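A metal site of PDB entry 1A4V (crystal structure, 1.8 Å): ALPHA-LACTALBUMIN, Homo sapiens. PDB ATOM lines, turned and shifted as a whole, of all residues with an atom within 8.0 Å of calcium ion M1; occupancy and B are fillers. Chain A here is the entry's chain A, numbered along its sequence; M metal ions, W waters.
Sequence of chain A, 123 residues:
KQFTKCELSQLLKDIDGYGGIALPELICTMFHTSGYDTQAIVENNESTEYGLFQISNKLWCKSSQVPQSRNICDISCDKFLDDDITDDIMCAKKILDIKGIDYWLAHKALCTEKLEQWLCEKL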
ATOM      1  N   THR A  38       1.464  32.706 -13.896  1.00  0.00           N
ATOM      2  CA  THR A  38       1.968  31.327 -14.120  1.00  0.00           C
ATOM      3  C   THR A  38       1.509  30.343 -13.035  1.00  0.00           C
ATOM      4  O   THR A  38       1.661  29.130 -13.194  1.00  0.00           O
ATOM      5  CB  THR A  38       3.504  31.270 -14.166  1.00  0.00           C
ATOM      6  OG1 THR A  38       4.053  31.588 -12.884  1.00  0.00           O
ATOM      7  CG2 THR A  38       4.041  32.244 -15.202  1.00  0.00           C
ATOM      8  N   ILE A  75       3.483  15.467 -20.240  1.00  0.00           N
ATOM      9  CA  ILE A  75       4.143  16.255 -19.213  1.00  0.00           C
ATOM     10  C   ILE A  75       3.240  16.328 -17.978  1.00  0.00           C
ATOM     11  O   ILE A  75       2.027  16.190 -18.097  1.00  0.00           O
ATOM     12  CB  ILE A  75       4.457  17.660 -19.781  1.00  0.00           C
ATOM     13  CG1 ILE A  75       5.388  18.475 -18.859  1.00  0.00           C
ATOM     14  CG2 ILE A  75       3.142  18.412 -20.107  1.00  0.00           C
ATOM     15  CD1 ILE A  75       5.916  19.792 -19.504  1.00  0.00           C
ATOM     16  N   SER A  76       3.817  16.384 -16.799  1.00  0.00           N
ATOM     17  CA  SER A  76       2.973  16.460 -15.647  1.00  0.00           C
ATOM     18  C   SER A  76       2.566  17.932 -15.469  1.00  0.00           C
ATOM     19  O   SER A  76       3.311  18.858 -15.800  1.00  0.00           O
ATOM     20  CB  SER A  76       3.615  15.874 -14.406  1.00  0.00           C
ATOM     21  OG  SER A  76       4.795  16.540 -14.045  1.00  0.00           O
ATOM     22  N   CYS A  77       1.357  18.117 -14.932  1.00  0.00           N
ATOM     23  CA  CYS A  77       0.783  19.427 -14.757  1.00  0.00           C
ATOM     24  C   CYS A  77       1.550  20.386 -13.870  1.00  0.00           C
ATOM     25  O   CYS A  77       1.423  21.602 -14.052  1.00  0.00           O
ATOM     26  CB  CYS A  77      -0.661  19.301 -14.309  1.00  0.00           C
ATOM     27  SG  CYS A  77      -1.721  18.233 -15.322  1.00  0.00           S
ATOM     28  N   ASP A  78       2.416  19.881 -12.966  1.00  0.00           N
ATOM     29  CA  ASP A  78       3.173  20.799 -12.093  1.00  0.00           C
ATOM     30  C   ASP A  78       4.132  21.716 -12.930  1.00  0.00           C
ATOM     31  O   ASP A  78       4.520  22.781 -12.495  1.00  0.00           O
ATOM     32  CB  ASP A  78       3.914  20.043 -10.969  1.00  0.00           C
ATOM     33  CG  ASP A  78       5.013  19.088 -11.490  1.00  0.00           C
ATOM     34  OD1 ASP A  78       4.695  17.925 -11.816  1.00  0.00           O
ATOM     35  OD2 ASP A  78       6.179  19.512 -11.627  1.00  0.00           O
ATOM     36  N   LYS A  79       4.549  21.225 -14.096  1.00  0.00           N
ATOM     37  CA  LYS A  79       5.467  21.979 -14.963  1.00  0.00           C
ATOM     38  C   LYS A  79       4.829  23.233 -15.540  1.00  0.00           C
ATOM     39  O   LYS A  79       5.497  24.010 -16.202  1.00  0.00           O
ATOM     40  CB  LYS A  79       6.000  21.136 -16.112  1.00  0.00           C
ATOM     41  CG  LYS A  79       6.995  20.084 -15.711  1.00  0.00           C
ATOM     42  CD  LYS A  79       8.385  20.646 -15.603  1.00  0.00           C
ATOM     43  CE  LYS A  79       9.314  19.474 -15.294  1.00  0.00           C
ATOM     44  NZ  LYS A  79      10.593  20.025 -14.880  1.00  0.00           N
ATOM     45  N   PHE A  80       3.532  23.385 -15.341  1.00  0.00           N
ATOM     46  CA  PHE A  80       2.840  24.552 -15.848  1.00  0.00           C
ATOM     47  C   PHE A  80       2.679  25.609 -14.752  1.00  0.00           C
ATOM     48  O   PHE A  80       1.993  26.618 -14.965  1.00  0.00           O
ATOM     49  CB  PHE A  80       1.457  24.154 -16.367  1.00  0.00           C
ATOM     50  CG  PHE A  80       1.514  23.334 -17.611  1.00  0.00           C
ATOM     51  CD1 PHE A  80       2.628  23.374 -18.452  1.00  0.00           C
ATOM     52  CD2 PHE A  80       0.468  22.484 -17.925  1.00  0.00           C
ATOM     53  CE1 PHE A  80       2.736  22.560 -19.565  1.00  0.00           C
ATOM     54  CE2 PHE A  80       0.537  21.646 -19.040  1.00  0.00           C
ATOM     55  CZ  PHE A  80       1.671  21.684 -19.860  1.00  0.00           C
ATOM     56  N   LEU A  81       3.206  25.323 -13.560  1.00  0.00           N
ATOM     57  CA  LEU A  81       3.117  26.220 -12.376  1.00  0.00           C
ATOM     58  C   LEU A  81       4.386  26.948 -12.002  1.00  0.00           C
ATOM     59  O   LEU A  81       4.339  27.902 -11.220  1.00  0.00           O
ATOM     60  CB  LEU A  81       2.598  25.468 -11.141  1.00  0.00           C
ATOM     61  CG  LEU A  81       1.258  24.743 -11.334  1.00  0.00           C
ATOM     62  CD1 LEU A  81       0.861  23.935 -10.103  1.00  0.00           C
ATOM     63  CD2 LEU A  81       0.167  25.774 -11.640  1.00  0.00           C
ATOM     64  N   ASP A  82       5.499  26.565 -12.649  1.00  0.00           N
ATOM     65  CA  ASP A  82       6.803  27.185 -12.450  1.00  0.00           C
ATOM     66  C   ASP A  82       7.002  28.494 -13.290  1.00  0.00           C
ATOM     67  O   ASP A  82       6.131  28.903 -14.031  1.00  0.00           O
ATOM     68  CB  ASP A  82       7.942  26.164 -12.665  1.00  0.00           C
ATOM     69  CG  ASP A  82       8.059  25.648 -14.129  1.00  0.00           C
ATOM     70  OD1 ASP A  82       7.581  26.344 -15.024  1.00  0.00           O
ATOM     71  OD2 ASP A  82       8.641  24.555 -14.362  1.00  0.00           O
ATOM     72  N   ASP A  83       8.140  29.143 -13.170  1.00  0.00           N
ATOM     73  CA  ASP A  83       8.362  30.385 -13.885  1.00  0.00           C
ATOM     74  C   ASP A  83       8.670  30.276 -15.357  1.00  0.00           C
ATOM     75  O   ASP A  83       8.509  31.277 -16.076  1.00  0.00           O
ATOM     76  CB  ASP A  83       9.485  31.184 -13.243  1.00  0.00           C
ATOM     77  CG  ASP A  83       9.220  31.589 -11.820  1.00  0.00           C
ATOM     78  OD1 ASP A  83       8.097  31.420 -11.316  1.00  0.00           O
ATOM     79  OD2 ASP A  83      10.184  32.095 -11.213  1.00  0.00           O
ATOM     80  N   ASP A  84       9.166  29.103 -15.809  1.00  0.00           N
ATOM     81  CA  ASP A  84       9.519  28.884 -17.232  1.00  0.00           C
ATOM     82  C   ASP A  84       8.293  28.513 -18.099  1.00  0.00           C
ATOM     83  O   ASP A  84       7.772  27.430 -17.955  1.00  0.00           O
ATOM     84  CB  ASP A  84      10.552  27.801 -17.320  1.00  0.00           C
ATOM     85  CG  ASP A  84      11.113  27.649 -18.713  1.00  0.00           C
ATOM     86  OD1 ASP A  84      10.805  28.498 -19.549  1.00  0.00           O
ATOM     87  OD2 ASP A  84      11.880  26.705 -18.994  1.00  0.00           O
ATOM     88  N   ILE A  85       7.775  29.438 -18.915  1.00  0.00           N
ATOM     89  CA  ILE A  85       6.607  29.155 -19.769  1.00  0.00           C
ATOM     90  C   ILE A  85       6.972  28.473 -21.113  1.00  0.00           C
ATOM     91  O   ILE A  85       6.115  28.234 -21.968  1.00  0.00           O
ATOM     92  CB  ILE A  85       5.691  30.437 -19.994  1.00  0.00           C
ATOM     93  CG1 ILE A  85       6.465  31.529 -20.747  1.00  0.00           C
ATOM     94  CG2 ILE A  85       5.165  30.984 -18.634  1.00  0.00           C
ATOM     95  CD1 ILE A  85       5.660  32.713 -21.082  1.00  0.00           C
ATOM     96  N   THR A  86       8.226  28.082 -21.265  1.00  0.00           N
ATOM     97  CA  THR A  86       8.637  27.455 -22.528  1.00  0.00           C
ATOM     98  C   THR A  86       7.821  26.204 -22.832  1.00  0.00           C
ATOM     99  O   THR A  86       7.253  26.055 -23.921  1.00  0.00           O
ATOM    100  CB  THR A  86      10.201  27.207 -22.629  1.00  0.00           C
ATOM    101  OG1 THR A  86      10.934  28.446 -22.519  1.00  0.00           O
ATOM    102  CG2 THR A  86      10.558  26.564 -24.004  1.00  0.00           C
ATOM    103  N   ASP A  87       7.784  25.289 -21.868  1.00  0.00           N
ATOM    104  CA  ASP A  87       7.010  24.111 -22.023  1.00  0.00           C
ATOM    105  C   ASP A  87       5.498  24.316 -22.085  1.00  0.00           C
ATOM    106  O   ASP A  87       4.816  23.593 -22.792  1.00  0.00           O
ATOM    107  CB  ASP A  87       7.462  23.029 -21.053  1.00  0.00           C
ATOM    108  CG  ASP A  87       7.346  23.408 -19.580  1.00  0.00           C
ATOM    109  OD1 ASP A  87       6.661  24.358 -19.256  1.00  0.00           O
ATOM    110  OD2 ASP A  87       7.951  22.715 -18.744  1.00  0.00           O
ATOM    111  N   ASP A  88       4.988  25.351 -21.437  1.00  0.00           N
ATOM    112  CA  ASP A  88       3.577  25.702 -21.476  1.00  0.00           C
ATOM    113  C   ASP A  88       3.260  26.084 -22.964  1.00  0.00           C
ATOM    114  O   ASP A  88       2.198  25.751 -23.487  1.00  0.00           O
ATOM    115  CB  ASP A  88       3.322  26.971 -20.595  1.00  0.00           C
ATOM    116  CG  ASP A  88       3.654  26.767 -19.135  1.00  0.00           C
ATOM    117  OD1 ASP A  88       4.773  26.366 -18.856  1.00  0.00           O
ATOM    118  OD2 ASP A  88       2.815  26.991 -18.250  1.00  0.00           O
ATOM    119  N   ILE A  89       4.155  26.864 -23.586  1.00  0.00           N
ATOM    120  CA  ILE A  89       3.994  27.284 -24.974  1.00  0.00           C
ATOM    121  C   ILE A  89       3.994  26.054 -25.901  1.00  0.00           C
ATOM    122  O   ILE A  89       3.197  25.946 -26.838  1.00  0.00           O
ATOM    123  CB  ILE A  89       5.126  28.276 -25.376  1.00  0.00           C
ATOM    124  CG1 ILE A  89       5.067  29.560 -24.550  1.00  0.00           C
ATOM    125  CG2 ILE A  89       5.029  28.648 -26.843  1.00  0.00           C
ATOM    126  CD1 ILE A  89       6.199  30.476 -24.922  1.00  0.00           C
HETATM  127 CA    CA M   1       6.571  25.756 -17.202  1.00  0.00          CA
HETATM  128 CA    CA M   2       5.471  30.400 -10.953  1.00  0.00          CA
HETATM  129  O   HOH W   1       8.709  24.467 -17.028  1.00  0.00           O
HETATM  130  O   HOH W   2       4.980  27.448 -16.136  1.00  0.00           O
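The side-chain hydroxyl (OG1) of Thr 86 is in hydrogen-bond range of the side-chain carboxylate (OD1) of Asp 84, 3.0 Å away.
Water W1 bridges OD2 of Asp 87 (2.6 Å) and OD2 of Asp 82 (2.7 Å).
O of Asp 84 binds calcium ion M1 (2.2 Å).
O of Lys 79 is bound to calcium ion M1.
OD1 of Asp 82 is bound to calcium ion M1, 2.5 Å away.
The side-chain carboxylate (OD1) of Asp 87 binds calcium ion M1 (2.5 Å).
Water W1 is bound to calcium ion M1, at 2.5 Å.
Calcium ion M1 is bound by the side-chain carboxylate (OD1) of Asp 88 (2.5 Å).
Calcium ion M1 is bound by water W2.
Calcium ion M1 has seven donor atoms within binding distance.
Five residues have an atom within 4 Å of calcium ion M1: Lys 79, Asp 82, Asp 84, Asp 87 and Asp 88.
The nearest printed residue that does not touch calcium ion M1 is Phe 80 (4.1 Å).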
